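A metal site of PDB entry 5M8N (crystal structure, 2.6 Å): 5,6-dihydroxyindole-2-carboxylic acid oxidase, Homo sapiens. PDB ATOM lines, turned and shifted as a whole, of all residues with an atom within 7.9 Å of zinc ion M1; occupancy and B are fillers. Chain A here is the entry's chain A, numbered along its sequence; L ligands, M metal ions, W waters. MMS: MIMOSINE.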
ATOM      1  N   HIS A 168       8.469  33.270  29.256  1.00  0.00           N
ATOM      2  CA  HIS A 168       9.115  32.053  28.791  1.00  0.00           C
ATOM      3  C   HIS A 168      10.408  31.802  29.577  1.00  0.00           C
ATOM      4  O   HIS A 168      10.692  30.657  29.948  1.00  0.00           O
ATOM      5  CB  HIS A 168       9.392  32.174  27.292  1.00  0.00           C
ATOM      6  CG  HIS A 168       9.864  30.917  26.646  1.00  0.00           C
ATOM      7  ND1 HIS A 168      11.199  30.680  26.400  1.00  0.00           N
ATOM      8  CD2 HIS A 168       9.192  29.841  26.183  1.00  0.00           C
ATOM      9  CE1 HIS A 168      11.325  29.506  25.797  1.00  0.00           C
ATOM     10  NE2 HIS A 168      10.120  28.974  25.667  1.00  0.00           N
ATOM     11  N   SER A 190       7.724  24.677  31.264  1.00  0.00           N
ATOM     12  CA  SER A 190       7.114  24.820  29.944  1.00  0.00           C
ATOM     13  C   SER A 190       7.651  23.864  28.879  1.00  0.00           C
ATOM     14  O   SER A 190       7.161  23.903  27.733  1.00  0.00           O
ATOM     15  CB  SER A 190       7.262  26.265  29.456  1.00  0.00           C
ATOM     16  OG  SER A 190       8.535  26.783  29.794  1.00  0.00           O
ATOM     17  N   HIS A 191       8.630  23.028  29.218  1.00  0.00           N
ATOM     18  CA  HIS A 191       9.197  22.061  28.287  1.00  0.00           C
ATOM     19  C   HIS A 191       9.398  20.739  29.000  1.00  0.00           C
ATOM     20  O   HIS A 191       9.270  20.643  30.217  1.00  0.00           O
ATOM     21  CB  HIS A 191      10.539  22.562  27.716  1.00  0.00           C
ATOM     22  CG  HIS A 191      10.478  23.926  27.147  1.00  0.00           C
ATOM     23  ND1 HIS A 191      10.664  25.062  27.913  1.00  0.00           N
ATOM     24  CD2 HIS A 191      10.170  24.351  25.893  1.00  0.00           C
ATOM     25  CE1 HIS A 191      10.507  26.128  27.146  1.00  0.00           C
ATOM     26  NE2 HIS A 191      10.207  25.729  25.921  1.00  0.00           N
ATOM     27  N   PHE A 196       4.047  21.355  27.882  1.00  0.00           N
ATOM     28  CA  PHE A 196       4.650  22.018  26.726  1.00  0.00           C
ATOM     29  C   PHE A 196       3.632  22.632  25.748  1.00  0.00           C
ATOM     30  O   PHE A 196       3.619  23.842  25.511  1.00  0.00           O
ATOM     31  CB  PHE A 196       5.563  21.002  26.020  1.00  0.00           C
ATOM     32  CG  PHE A 196       6.124  21.488  24.726  1.00  0.00           C
ATOM     33  CD1 PHE A 196       6.981  22.551  24.689  1.00  0.00           C
ATOM     34  CD2 PHE A 196       5.793  20.866  23.529  1.00  0.00           C
ATOM     35  CE1 PHE A 196       7.511  23.008  23.476  1.00  0.00           C
ATOM     36  CE2 PHE A 196       6.302  21.298  22.321  1.00  0.00           C
ATOM     37  CZ  PHE A 196       7.167  22.375  22.289  1.00  0.00           C
ATOM     38  N   HIS A 200       2.709  26.706  25.564  1.00  0.00           N
ATOM     39  CA  HIS A 200       3.021  27.563  24.428  1.00  0.00           C
ATOM     40  C   HIS A 200       1.758  28.035  23.723  1.00  0.00           C
ATOM     41  O   HIS A 200       1.768  29.130  23.155  1.00  0.00           O
ATOM     42  CB  HIS A 200       3.963  26.830  23.484  1.00  0.00           C
ATOM     43  CG  HIS A 200       5.341  26.671  24.060  1.00  0.00           C
ATOM     44  ND1 HIS A 200       5.624  25.808  25.105  1.00  0.00           N
ATOM     45  CD2 HIS A 200       6.505  27.327  23.798  1.00  0.00           C
ATOM     46  CE1 HIS A 200       6.900  25.899  25.424  1.00  0.00           C
ATOM     47  NE2 HIS A 200       7.455  26.822  24.648  1.00  0.00           N
ATOM     48  N   GLU A 336       7.299  18.005  20.279  1.00  0.00           N
ATOM     49  CA  GLU A 336       8.337  18.776  20.963  1.00  0.00           C
ATOM     50  C   GLU A 336       9.710  18.475  20.401  1.00  0.00           C
ATOM     51  O   GLU A 336      10.509  19.385  20.158  1.00  0.00           O
ATOM     52  CB  GLU A 336       8.330  18.533  22.474  1.00  0.00           C
ATOM     53  CG  GLU A 336       9.371  19.342  23.237  1.00  0.00           C
ATOM     54  CD  GLU A 336       9.108  19.410  24.764  1.00  0.00           C
ATOM     55  OE1 GLU A 336       8.175  18.721  25.249  1.00  0.00           O
ATOM     56  OE2 GLU A 336       9.844  20.123  25.505  1.00  0.00           O
ATOM     57  N   HIS A 353       9.802  20.304  16.617  1.00  0.00           N
ATOM     58  CA  HIS A 353       9.874  21.616  17.272  1.00  0.00           C
ATOM     59  C   HIS A 353      11.285  21.960  17.768  1.00  0.00           C
ATOM     60  O   HIS A 353      11.709  23.120  17.675  1.00  0.00           O
ATOM     61  CB  HIS A 353       8.904  21.696  18.440  1.00  0.00           C
ATOM     62  CG  HIS A 353       9.294  22.700  19.480  1.00  0.00           C
ATOM     63  ND1 HIS A 353       9.989  22.352  20.628  1.00  0.00           N
ATOM     64  CD2 HIS A 353       9.060  24.031  19.576  1.00  0.00           C
ATOM     65  CE1 HIS A 353      10.163  23.417  21.378  1.00  0.00           C
ATOM     66  NE2 HIS A 353       9.613  24.455  20.762  1.00  0.00           N
ATOM     67  N   ASN A 354      12.003  20.980  18.341  1.00  0.00           N
ATOM     68  CA  ASN A 354      13.333  21.263  18.882  1.00  0.00           C
ATOM     69  C   ASN A 354      14.362  21.418  17.770  1.00  0.00           C
ATOM     70  O   ASN A 354      15.270  22.241  17.886  1.00  0.00           O
ATOM     71  CB  ASN A 354      13.790  20.172  19.850  1.00  0.00           C
ATOM     72  CG  ASN A 354      13.154  20.288  21.228  1.00  0.00           C
ATOM     73  OD1 ASN A 354      12.727  21.371  21.672  1.00  0.00           O
ATOM     74  ND2 ASN A 354      13.090  19.160  21.939  1.00  0.00           N
ATOM     75  N   ALA A 356      13.695  22.567  14.692  1.00  0.00           N
ATOM     76  CA  ALA A 356      13.498  23.920  14.178  1.00  0.00           C
ATOM     77  C   ALA A 356      14.256  24.936  15.021  1.00  0.00           C
ATOM     78  O   ALA A 356      14.840  25.884  14.488  1.00  0.00           O
ATOM     79  CB  ALA A 356      12.015  24.267  14.154  1.00  0.00           C
ATOM     80  N   HIS A 357      14.258  24.771  16.349  1.00  0.00           N
ATOM     81  CA  HIS A 357      14.913  25.747  17.218  1.00  0.00           C
ATOM     82  C   HIS A 357      16.411  25.756  16.988  1.00  0.00           C
ATOM     83  O   HIS A 357      17.021  26.802  16.768  1.00  0.00           O
ATOM     84  CB  HIS A 357      14.613  25.455  18.695  1.00  0.00           C
ATOM     85  CG  HIS A 357      13.423  26.202  19.231  1.00  0.00           C
ATOM     86  ND1 HIS A 357      13.419  27.573  19.389  1.00  0.00           N
ATOM     87  CD2 HIS A 357      12.209  25.766  19.646  1.00  0.00           C
ATOM     88  CE1 HIS A 357      12.250  27.951  19.877  1.00  0.00           C
ATOM     89  NE2 HIS A 357      11.498  26.874  20.035  1.00  0.00           N
ATOM     90  N   GLY A 364      17.615  31.932  18.937  1.00  0.00           N
ATOM     91  CA  GLY A 364      16.407  31.136  18.929  1.00  0.00           C
ATOM     92  C   GLY A 364      16.610  29.698  19.290  1.00  0.00           C
ATOM     93  O   GLY A 364      15.633  28.960  19.438  1.00  0.00           O
ATOM     94  N   THR A 367      16.989  27.972  25.204  1.00  0.00           N
ATOM     95  CA  THR A 367      15.684  27.966  25.798  1.00  0.00           C
ATOM     96  C   THR A 367      15.334  29.174  26.604  1.00  0.00           C
ATOM     97  O   THR A 367      14.246  29.659  26.508  1.00  0.00           O
ATOM     98  CB  THR A 367      15.488  26.720  26.640  1.00  0.00           C
ATOM     99  OG1 THR A 367      16.056  25.637  25.935  1.00  0.00           O
ATOM    100  CG2 THR A 367      14.044  26.446  26.874  1.00  0.00           C
ATOM    101  N   SER A 370      15.079  32.082  23.568  1.00  0.00           N
ATOM    102  CA  SER A 370      14.621  31.917  22.191  1.00  0.00           C
ATOM    103  C   SER A 370      13.494  32.855  21.756  1.00  0.00           C
ATOM    104  O   SER A 370      13.489  33.210  20.567  1.00  0.00           O
ATOM    105  CB  SER A 370      14.238  30.460  21.949  1.00  0.00           C
ATOM    106  OG  SER A 370      13.215  30.083  22.839  1.00  0.00           O
ATOM    107  N   PRO A 371      12.532  33.267  22.583  1.00  0.00           N
ATOM    108  CA  PRO A 371      11.500  34.197  22.063  1.00  0.00           C
ATOM    109  C   PRO A 371      12.064  35.537  21.657  1.00  0.00           C
ATOM    110  O   PRO A 371      11.346  36.323  21.030  1.00  0.00           O
ATOM    111  CB  PRO A 371      10.508  34.324  23.237  1.00  0.00           C
ATOM    112  CG  PRO A 371      10.727  33.108  24.028  1.00  0.00           C
ATOM    113  CD  PRO A 371      12.221  32.887  23.976  1.00  0.00           C
ATOM    114  N   PHE A 376      10.357  32.727  16.670  1.00  0.00           N
ATOM    115  CA  PHE A 376       9.744  31.941  17.740  1.00  0.00           C
ATOM    116  C   PHE A 376       8.237  31.898  17.615  1.00  0.00           C
ATOM    117  O   PHE A 376       7.626  30.829  17.647  1.00  0.00           O
ATOM    118  CB  PHE A 376      10.141  32.536  19.094  1.00  0.00           C
ATOM    119  CG  PHE A 376       9.691  31.722  20.246  1.00  0.00           C
ATOM    120  CD1 PHE A 376       8.437  31.944  20.823  1.00  0.00           C
ATOM    121  CD2 PHE A 376      10.517  30.744  20.776  1.00  0.00           C
ATOM    122  CE1 PHE A 376       8.022  31.187  21.891  1.00  0.00           C
ATOM    123  CE2 PHE A 376      10.115  29.993  21.846  1.00  0.00           C
ATOM    124  CZ  PHE A 376       8.857  30.212  22.399  1.00  0.00           C
ATOM    125  N   LEU A 379       7.491  29.851  14.658  1.00  0.00           N
ATOM    126  CA  LEU A 379       7.856  28.466  14.981  1.00  0.00           C
ATOM    127  C   LEU A 379       6.811  27.850  15.890  1.00  0.00           C
ATOM    128  O   LEU A 379       6.428  26.683  15.730  1.00  0.00           O
ATOM    129  CB  LEU A 379       9.244  28.442  15.617  1.00  0.00           C
ATOM    130  CG  LEU A 379      10.050  27.141  15.827  1.00  0.00           C
ATOM    131  CD1 LEU A 379      11.386  27.489  16.443  1.00  0.00           C
ATOM    132  CD2 LEU A 379       9.350  26.030  16.664  1.00  0.00           C
ATOM    133  N   HIS A 380       6.266  28.631  16.801  1.00  0.00           N
ATOM    134  CA  HIS A 380       5.332  28.062  17.757  1.00  0.00           C
ATOM    135  C   HIS A 380       3.882  28.105  17.326  1.00  0.00           C
ATOM    136  O   HIS A 380       3.107  27.280  17.830  1.00  0.00           O
ATOM    137  CB  HIS A 380       5.507  28.739  19.110  1.00  0.00           C
ATOM    138  CG  HIS A 380       6.539  28.060  19.926  1.00  0.00           C
ATOM    139  ND1 HIS A 380       6.301  26.860  20.550  1.00  0.00           N
ATOM    140  CD2 HIS A 380       7.855  28.323  20.103  1.00  0.00           C
ATOM    141  CE1 HIS A 380       7.411  26.443  21.124  1.00  0.00           C
ATOM    142  NE2 HIS A 380       8.368  27.316  20.874  1.00  0.00           N
ATOM    143  N   THR A 383       3.602  24.997  15.598  1.00  0.00           N
ATOM    144  CA  THR A 383       3.540  23.909  16.590  1.00  0.00           C
ATOM    145  C   THR A 383       2.146  23.791  17.169  1.00  0.00           C
ATOM    146  O   THR A 383       1.623  22.680  17.310  1.00  0.00           O
ATOM    147  CB  THR A 383       4.565  24.167  17.713  1.00  0.00           C
ATOM    148  OG1 THR A 383       5.889  24.276  17.156  1.00  0.00           O
ATOM    149  CG2 THR A 383       4.577  23.038  18.745  1.00  0.00           C
HETATM  150  O4  MMS L   1      12.228  25.110  23.565  1.00  0.00           O
HETATM  151  C1  MMS L   1      17.123  20.805  23.070  1.00  0.00           C
HETATM  152  O1  MMS L   1      16.923  20.266  21.996  1.00  0.00           O
HETATM  153  O2  MMS L   1      17.910  20.321  23.906  1.00  0.00           O
HETATM  154  N1  MMS L   1      17.326  22.782  24.269  1.00  0.00           N
HETATM  155  C2  MMS L   1      16.420  22.098  23.385  1.00  0.00           C
HETATM  156  C3  MMS L   1      16.146  22.851  22.090  1.00  0.00           C
HETATM  157  N2  MMS L   1      15.470  24.078  22.368  1.00  0.00           N
HETATM  158  C8  MMS L   1      14.099  24.036  22.833  1.00  0.00           C
HETATM  159  C4  MMS L   1      16.114  25.384  22.199  1.00  0.00           C
HETATM  160  C7  MMS L   1      13.485  25.145  23.094  1.00  0.00           C
HETATM  161  C5  MMS L   1      15.477  26.495  22.455  1.00  0.00           C
HETATM  162  C6  MMS L   1      14.105  26.465  22.948  1.00  0.00           C
HETATM  163  O3  MMS L   1      13.499  27.429  23.215  1.00  0.00           O
HETATM  164 ZN    ZN M   1      10.009  26.295  21.397  1.00  0.00          ZN
HETATM  165 ZN    ZN M   2       9.463  27.299  24.837  1.00  0.00          ZN
HETATM  166  O   HOH W   1      10.695  26.931  23.190  1.00  0.00           O
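Zinc ion M1 is bound by a ring nitrogen (NE2) of His 353 (2.0 Å), a ring nitrogen (NE2) of His 380 (2.0 Å), water W1 (2.0 Å) and a ring nitrogen (NE2) of His 357 (2.1 Å).
Zinc ion M1 has four donor atoms within binding distance.
Merely in contact with zinc ion M1: Phe 376.
Of the 18 residues printed, 4 come within 4 Å of zinc ion M1.
The nearest printed residue that does not touch zinc ion M1 is His 200 (4.2 Å).
An oxygen (O4) of the ligand sits close to a ring nitrogen (NE2) of His 191.
An oxygen (O3) of the ligand lies within hydrogen-bond range of the side-chain hydroxyl (OG) of Ser 370 (2.7 Å).
ND1 of His 353 is in hydrogen-bond range of OD1 of Asn 354.
ND1 of His 353 is in hydrogen-bond range of O of Glu 336.
The backbone carbonyl oxygen (O) of Gly 364 lies within hydrogen-bond range of a ring nitrogen (ND1) of His 357, 2.6 Å away.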
